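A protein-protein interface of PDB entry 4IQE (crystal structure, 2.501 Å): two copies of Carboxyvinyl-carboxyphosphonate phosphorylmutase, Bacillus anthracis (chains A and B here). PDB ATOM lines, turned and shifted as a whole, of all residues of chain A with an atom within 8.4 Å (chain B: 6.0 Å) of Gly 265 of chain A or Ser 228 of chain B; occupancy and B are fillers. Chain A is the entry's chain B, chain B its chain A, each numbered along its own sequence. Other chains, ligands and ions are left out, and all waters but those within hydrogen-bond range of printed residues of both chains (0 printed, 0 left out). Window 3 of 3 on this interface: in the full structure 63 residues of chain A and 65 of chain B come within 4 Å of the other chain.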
ATOM      1  N   VAL A 257       1.842 -13.854 -18.043  1.00  0.00           N
ATOM      2  CA  VAL A 257       1.557 -13.095 -19.255  1.00  0.00           C
ATOM      3  C   VAL A 257       1.537 -11.585 -19.006  1.00  0.00           C
ATOM      4  O   VAL A 257       1.825 -10.801 -19.907  1.00  0.00           O
ATOM      5  CB  VAL A 257       0.245 -13.562 -19.934  1.00  0.00           C
ATOM      6  CG1 VAL A 257      -0.973 -13.038 -19.186  1.00  0.00           C
ATOM      7  CG2 VAL A 257       0.216 -13.125 -21.391  1.00  0.00           C
ATOM      8  N   PHE A 258       1.215 -11.181 -17.780  1.00  0.00           N
ATOM      9  CA  PHE A 258       1.226  -9.767 -17.420  1.00  0.00           C
ATOM     10  C   PHE A 258       2.651  -9.261 -17.241  1.00  0.00           C
ATOM     11  O   PHE A 258       3.009  -8.197 -17.746  1.00  0.00           O
ATOM     12  CB  PHE A 258       0.420  -9.517 -16.144  1.00  0.00           C
ATOM     13  CG  PHE A 258      -1.066  -9.511 -16.357  1.00  0.00           C
ATOM     14  CD1 PHE A 258      -1.598  -9.269 -17.613  1.00  0.00           C
ATOM     15  CD2 PHE A 258      -1.930  -9.743 -15.301  1.00  0.00           C
ATOM     16  CE1 PHE A 258      -2.967  -9.260 -17.812  1.00  0.00           C
ATOM     17  CE2 PHE A 258      -3.298  -9.737 -15.493  1.00  0.00           C
ATOM     18  CZ  PHE A 258      -3.818  -9.495 -16.749  1.00  0.00           C
ATOM     19  N   THR A 259       3.458 -10.031 -16.514  1.00  0.00           N
ATOM     20  CA  THR A 259       4.863  -9.700 -16.307  1.00  0.00           C
ATOM     21  C   THR A 259       5.579  -9.621 -17.648  1.00  0.00           C
ATOM     22  O   THR A 259       6.451  -8.776 -17.851  1.00  0.00           O
ATOM     23  CB  THR A 259       5.562 -10.740 -15.409  1.00  0.00           C
ATOM     24  OG1 THR A 259       4.873 -10.833 -14.156  1.00  0.00           O
ATOM     25  CG2 THR A 259       7.011 -10.349 -15.157  1.00  0.00           C
ATOM     26  N   LEU A 260       5.196 -10.505 -18.563  1.00  0.00           N
ATOM     27  CA  LEU A 260       5.725 -10.483 -19.918  1.00  0.00           C
ATOM     28  C   LEU A 260       5.367  -9.171 -20.601  1.00  0.00           C
ATOM     29  O   LEU A 260       6.240  -8.461 -21.094  1.00  0.00           O
ATOM     30  CB  LEU A 260       5.174 -11.657 -20.727  1.00  0.00           C
ATOM     31  CG  LEU A 260       5.525 -11.669 -22.216  1.00  0.00           C
ATOM     32  CD1 LEU A 260       7.029 -11.774 -22.413  1.00  0.00           C
ATOM     33  CD2 LEU A 260       4.806 -12.801 -22.931  1.00  0.00           C
ATOM     34  N   ILE A 261       4.078  -8.852 -20.616  1.00  0.00           N
ATOM     35  CA  ILE A 261       3.588  -7.637 -21.262  1.00  0.00           C
ATOM     36  C   ILE A 261       4.179  -6.372 -20.641  1.00  0.00           C
ATOM     37  O   ILE A 261       4.521  -5.425 -21.349  1.00  0.00           O
ATOM     38  CB  ILE A 261       2.045  -7.573 -21.234  1.00  0.00           C
ATOM     39  CG1 ILE A 261       1.460  -8.647 -22.152  1.00  0.00           C
ATOM     40  CG2 ILE A 261       1.548  -6.201 -21.658  1.00  0.00           C
ATOM     41  CD1 ILE A 261      -0.050  -8.720 -22.129  1.00  0.00           C
ATOM     42  N   LYS A 262       4.319  -6.364 -19.321  1.00  0.00           N
ATOM     43  CA  LYS A 262       4.849  -5.194 -18.629  1.00  0.00           C
ATOM     44  C   LYS A 262       6.349  -5.002 -18.858  1.00  0.00           C
ATOM     45  O   LYS A 262       6.823  -3.874 -18.990  1.00  0.00           O
ATOM     46  CB  LYS A 262       4.550  -5.269 -17.130  1.00  0.00           C
ATOM     47  CG  LYS A 262       4.974  -4.032 -16.351  1.00  0.00           C
ATOM     48  CD  LYS A 262       4.331  -2.775 -16.918  1.00  0.00           C
ATOM     49  CE  LYS A 262       4.749  -1.538 -16.135  1.00  0.00           C
ATOM     50  NZ  LYS A 262       6.227  -1.345 -16.145  1.00  0.00           N
ATOM     51  N   GLU A 263       7.093  -6.103 -18.910  1.00  0.00           N
ATOM     52  CA  GLU A 263       8.545  -6.035 -19.051  1.00  0.00           C
ATOM     53  C   GLU A 263       9.016  -6.053 -20.506  1.00  0.00           C
ATOM     54  O   GLU A 263      10.027  -5.439 -20.843  1.00  0.00           O
ATOM     55  CB  GLU A 263       9.220  -7.160 -18.259  1.00  0.00           C
ATOM     56  CG  GLU A 263       9.010  -7.069 -16.755  1.00  0.00           C
ATOM     57  CD  GLU A 263       9.795  -8.116 -15.991  1.00  0.00           C
ATOM     58  OE1 GLU A 263      10.610  -8.824 -16.618  1.00  0.00           O
ATOM     59  OE2 GLU A 263       9.597  -8.232 -14.763  1.00  0.00           O
ATOM     60  N   THR A 264       8.285  -6.756 -21.365  1.00  0.00           N
ATOM     61  CA  THR A 264       8.642  -6.844 -22.779  1.00  0.00           C
ATOM     62  C   THR A 264       7.908  -5.796 -23.615  1.00  0.00           C
ATOM     63  O   THR A 264       8.509  -5.127 -24.458  1.00  0.00           O
ATOM     64  CB  THR A 264       8.382  -8.259 -23.347  1.00  0.00           C
ATOM     65  OG1 THR A 264       9.443  -9.137 -22.950  1.00  0.00           O
ATOM     66  CG2 THR A 264       8.297  -8.235 -24.866  1.00  0.00           C
ATOM     67  N   GLY A 265       6.611  -5.650 -23.368  1.00  0.00           N
ATOM     68  CA  GLY A 265       5.794  -4.717 -24.121  1.00  0.00           C
ATOM     69  C   GLY A 265       4.912  -5.439 -25.117  1.00  0.00           C
ATOM     70  O   GLY A 265       4.236  -4.814 -25.933  1.00  0.00           O
ATOM     71  N   SER A 266       4.920  -6.765 -25.042  1.00  0.00           N
ATOM     72  CA  SER A 266       4.142  -7.595 -25.954  1.00  0.00           C
ATOM     73  C   SER A 266       3.847  -8.955 -25.330  1.00  0.00           C
ATOM     74  O   SER A 266       4.526  -9.375 -24.393  1.00  0.00           O
ATOM     75  CB  SER A 266       4.893  -7.778 -27.274  1.00  0.00           C
ATOM     76  OG  SER A 266       4.173  -8.619 -28.157  1.00  0.00           O
ATOM     77  N   GLN A 267       2.832  -9.637 -25.850  1.00  0.00           N
ATOM     78  CA  GLN A 267       2.480 -10.968 -25.363  1.00  0.00           C
ATOM     79  C   GLN A 267       2.907 -12.043 -26.358  1.00  0.00           C
ATOM     80  O   GLN A 267       2.425 -13.176 -26.308  1.00  0.00           O
ATOM     81  CB  GLN A 267       0.974 -11.067 -25.086  1.00  0.00           C
ATOM     82  CG  GLN A 267       0.085 -11.080 -26.327  1.00  0.00           C
ATOM     83  CD  GLN A 267      -0.244  -9.692 -26.841  1.00  0.00           C
ATOM     84  OE1 GLN A 267       0.645  -8.918 -27.195  1.00  0.00           O
ATOM     85  NE2 GLN A 267      -1.531  -9.370 -26.881  1.00  0.00           N
ATOM     86  N   LYS A 268       3.826 -11.681 -27.247  1.00  0.00           N
ATOM     87  CA  LYS A 268       4.249 -12.553 -28.340  1.00  0.00           C
ATOM     88  C   LYS A 268       4.843 -13.883 -27.877  1.00  0.00           C
ATOM     89  O   LYS A 268       4.654 -14.910 -28.526  1.00  0.00           O
ATOM     90  CB  LYS A 268       5.252 -11.828 -29.244  1.00  0.00           C
ATOM     91  CG  LYS A 268       6.511 -11.351 -28.531  1.00  0.00           C
ATOM     92  CD  LYS A 268       7.590 -10.937 -29.518  1.00  0.00           C
ATOM     93  CE  LYS A 268       7.135  -9.775 -30.383  1.00  0.00           C
ATOM     94  NZ  LYS A 268       8.191  -9.360 -31.349  1.00  0.00           N
ATOM     95  N   GLN B  32      -0.380   1.210 -21.270  1.00  0.00           N
ATOM     96  CA  GLN B  32      -0.696  -0.203 -21.445  1.00  0.00           C
ATOM     97  C   GLN B  32      -1.906  -0.577 -20.598  1.00  0.00           C
ATOM     98  O   GLN B  32      -1.876  -0.466 -19.373  1.00  0.00           O
ATOM     99  CB  GLN B  32       0.499  -1.083 -21.071  1.00  0.00           C
ATOM    100  CG  GLN B  32       1.696  -0.949 -21.998  1.00  0.00           C
ATOM    101  CD  GLN B  32       2.799  -1.935 -21.666  1.00  0.00           C
ATOM    102  OE1 GLN B  32       3.673  -1.654 -20.846  1.00  0.00           O
ATOM    103  NE2 GLN B  32       2.762  -3.099 -22.302  1.00  0.00           N
ATOM    104  N   TYR B 226       1.865  -8.203 -33.971  1.00  0.00           N
ATOM    105  CA  TYR B 226       2.244  -8.098 -32.567  1.00  0.00           C
ATOM    106  C   TYR B 226       3.318  -7.040 -32.327  1.00  0.00           C
ATOM    107  O   TYR B 226       4.451  -7.363 -31.971  1.00  0.00           O
ATOM    108  CB  TYR B 226       2.703  -9.459 -32.037  1.00  0.00           C
ATOM    109  CG  TYR B 226       1.658 -10.542 -32.177  1.00  0.00           C
ATOM    110  CD1 TYR B 226       0.697 -10.739 -31.194  1.00  0.00           C
ATOM    111  CD2 TYR B 226       1.630 -11.367 -33.295  1.00  0.00           C
ATOM    112  CE1 TYR B 226      -0.260 -11.728 -31.320  1.00  0.00           C
ATOM    113  CE2 TYR B 226       0.676 -12.357 -33.428  1.00  0.00           C
ATOM    114  CZ  TYR B 226      -0.266 -12.533 -32.439  1.00  0.00           C
ATOM    115  OH  TYR B 226      -1.219 -13.519 -32.569  1.00  0.00           O
ATOM    116  N   TYR B 227       2.953  -5.777 -32.526  1.00  0.00           N
ATOM    117  CA  TYR B 227       3.853  -4.670 -32.230  1.00  0.00           C
ATOM    118  C   TYR B 227       4.041  -4.554 -30.726  1.00  0.00           C
ATOM    119  O   TYR B 227       3.132  -4.864 -29.956  1.00  0.00           O
ATOM    120  CB  TYR B 227       3.292  -3.349 -32.761  1.00  0.00           C
ATOM    121  CG  TYR B 227       3.183  -3.257 -34.266  1.00  0.00           C
ATOM    122  CD1 TYR B 227       4.287  -2.939 -35.046  1.00  0.00           C
ATOM    123  CD2 TYR B 227       1.969  -3.464 -34.905  1.00  0.00           C
ATOM    124  CE1 TYR B 227       4.187  -2.845 -36.421  1.00  0.00           C
ATOM    125  CE2 TYR B 227       1.858  -3.371 -36.277  1.00  0.00           C
ATOM    126  CZ  TYR B 227       2.969  -3.061 -37.031  1.00  0.00           C
ATOM    127  OH  TYR B 227       2.857  -2.970 -38.397  1.00  0.00           O
ATOM    128  N   SER B 228       5.219  -4.106 -30.308  1.00  0.00           N
ATOM    129  CA  SER B 228       5.466  -3.842 -28.898  1.00  0.00           C
ATOM    130  C   SER B 228       4.761  -2.552 -28.501  1.00  0.00           C
ATOM    131  O   SER B 228       4.378  -1.760 -29.361  1.00  0.00           O
ATOM    132  CB  SER B 228       6.965  -3.731 -28.618  1.00  0.00           C
ATOM    133  OG  SER B 228       7.539  -2.649 -29.326  1.00  0.00           O
ATOM    134  N   ALA B 229       4.589  -2.347 -27.199  1.00  0.00           N
ATOM    135  CA  ALA B 229       3.943  -1.140 -26.696  1.00  0.00           C
ATOM    136  C   ALA B 229       4.740   0.102 -27.081  1.00  0.00           C
ATOM    137  O   ALA B 229       4.174   1.169 -27.313  1.00  0.00           O
ATOM    138  CB  ALA B 229       3.773  -1.219 -25.188  1.00  0.00           C
ATOM    139  N   GLU B 230       6.058  -0.050 -27.153  1.00  0.00           N
ATOM    140  CA  GLU B 230       6.938   1.045 -27.540  1.00  0.00           C
ATOM    141  C   GLU B 230       6.784   1.365 -29.023  1.00  0.00           C
ATOM    142  O   GLU B 230       6.951   2.509 -29.444  1.00  0.00           O
ATOM    143  CB  GLU B 230       8.394   0.694 -27.219  1.00  0.00           C
ATOM    144  CG  GLU B 230       9.376   1.833 -27.433  1.00  0.00           C
ATOM    145  CD  GLU B 230       9.165   2.978 -26.461  1.00  0.00           C
ATOM    146  OE1 GLU B 230       8.578   2.745 -25.382  1.00  0.00           O
ATOM    147  OE2 GLU B 230       9.586   4.111 -26.773  1.00  0.00           O
ATOM    148  N   GLU B 231       6.455   0.346 -29.812  1.00  0.00           N
ATOM    149  CA  GLU B 231       6.256   0.526 -31.247  1.00  0.00           C
ATOM    150  C   GLU B 231       4.942   1.236 -31.554  1.00  0.00           C
ATOM    151  O   GLU B 231       4.882   2.073 -32.454  1.00  0.00           O
ATOM    152  CB  GLU B 231       6.333  -0.816 -31.977  1.00  0.00           C
ATOM    153  CG  GLU B 231       7.753  -1.302 -32.221  1.00  0.00           C
ATOM    154  CD  GLU B 231       7.813  -2.761 -32.622  1.00  0.00           C
ATOM    155  OE1 GLU B 231       6.864  -3.506 -32.303  1.00  0.00           O
ATOM    156  OE2 GLU B 231       8.810  -3.167 -33.256  1.00  0.00           O
ATOM    157  N   PHE B 232       3.895   0.902 -30.807  1.00  0.00           N
ATOM    158  CA  PHE B 232       2.613   1.583 -30.953  1.00  0.00           C
ATOM    159  C   PHE B 232       2.752   3.058 -30.593  1.00  0.00           C
ATOM    160  O   PHE B 232       2.102   3.919 -31.185  1.00  0.00           O
ATOM    161  CB  PHE B 232       1.546   0.939 -30.065  1.00  0.00           C
ATOM    162  CG  PHE B 232       1.032  -0.374 -30.581  1.00  0.00           C
ATOM    163  CD1 PHE B 232       0.277  -0.431 -31.741  1.00  0.00           C
ATOM    164  CD2 PHE B 232       1.281  -1.549 -29.892  1.00  0.00           C
ATOM    165  CE1 PHE B 232      -0.205  -1.638 -32.213  1.00  0.00           C
ATOM    166  CE2 PHE B 232       0.800  -2.757 -30.357  1.00  0.00           C
ATOM    167  CZ  PHE B 232       0.055  -2.803 -31.520  1.00  0.00           C
ATOM    168  N   ALA B 233       3.611   3.340 -29.619  1.00  0.00           N
ATOM    169  CA  ALA B 233       3.817   4.700 -29.137  1.00  0.00           C
ATOM    170  C   ALA B 233       4.491   5.581 -30.184  1.00  0.00           C
ATOM    171  O   ALA B 233       4.229   6.780 -30.259  1.00  0.00           O
ATOM    172  CB  ALA B 233       4.627   4.688 -27.849  1.00  0.00           C
ATOM    173  N   TYR B 242      -4.972  -4.964 -24.173  1.00  0.00           N
ATOM    174  CA  TYR B 242      -4.810  -6.404 -24.332  1.00  0.00           C
ATOM    175  C   TYR B 242      -6.057  -7.068 -23.763  1.00  0.00           C
ATOM    176  O   TYR B 242      -6.034  -7.599 -22.653  1.00  0.00           O
ATOM    177  CB  TYR B 242      -3.562  -6.886 -23.595  1.00  0.00           C
ATOM    178  CG  TYR B 242      -2.325  -6.062 -23.875  1.00  0.00           C
ATOM    179  CD1 TYR B 242      -1.462  -6.395 -24.911  1.00  0.00           C
ATOM    180  CD2 TYR B 242      -2.020  -4.947 -23.103  1.00  0.00           C
ATOM    181  CE1 TYR B 242      -0.332  -5.642 -25.170  1.00  0.00           C
ATOM    182  CE2 TYR B 242      -0.894  -4.188 -23.357  1.00  0.00           C
ATOM    183  CZ  TYR B 242      -0.054  -4.541 -24.389  1.00  0.00           C
ATOM    184  OH  TYR B 242       1.069  -3.787 -24.642  1.00  0.00           O
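NE2 of Gln 32 of chain B is in hydrogen-bond range of O of Ile 261 of chain A.
N of Ala 229 of chain B sits at hydrogen-bond distance from O of Gly 265 of chain A.
NE2 of Gln 32 of chain B sits at hydrogen-bond distance from OH of Tyr 242 of chain B (3.0 Å).
The backbone NH of Ser 228 of chain B sits at hydrogen-bond distance from the side-chain carboxylate of Glu 231 of chain B, 2.7 Å away.
The side-chain hydroxyl (OG) of Ser 266 of chain A is in hydrogen-bond range of the backbone NH (N) of Lys 268 of chain A.
Among the printed residues, merely in contact across the chains: Gly 265 of chain A with Ser 228 of chain B, Gln 267 of chain A with Tyr 242 of chain B, Gly 265 of chain A with Tyr 242 of chain B, Ile 261 of chain A with Tyr 242 of chain B, Gly 265 of chain A with Gln 32 of chain B and Lys 268 of chain A with Tyr 226 of chain B.
Thr 259 of chain A touches none of the printed residues of chain B.
Leu 260 of chain A touches none of the printed residues of chain B.
Of the printed residues of chain B, Ile 261 of chain A touches Gln 32 and Tyr 242.
Gly 265 of chain A touches four residues of chain B.
Of the printed residues of chain B, Lys 268 of chain A touches Tyr 226 (3.9 Å).
Of the printed residues of chain A, Tyr 226 of chain B touches Lys 268.
Ser 228 of chain B touches just one residue of chain A: Gly 265.
Printed residues of chain A within 4 Å of Ala 229 of chain B: Gly 265 (2.8 Å).
Printed residues of chain A within 4 Å of Tyr 242 of chain B: Ile 261, Gly 265 and Gln 267.
The nearest residue of chain B that does not touch Gly 265 of chain A is Tyr 227 of chain B (4.2 Å).
The nearest residue of chain A that does not touch Ser 228 of chain B is Ser 266 of chain A (4.3 Å).
The nearest printed residue of chain A that does not touch Tyr 242 of chain B is Ser 266 of chain A (4.9 Å).
Hydrophobic or aromatic side chains of chain A that line the printed part of chain B: Ile 261.
Among the printed residues, 8 pairs touch across the chains.
No position is printed for both chains.
Of the 8 pairs that touch across the chains among the printed residues, none has its exchanged pair printed and touching as well.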
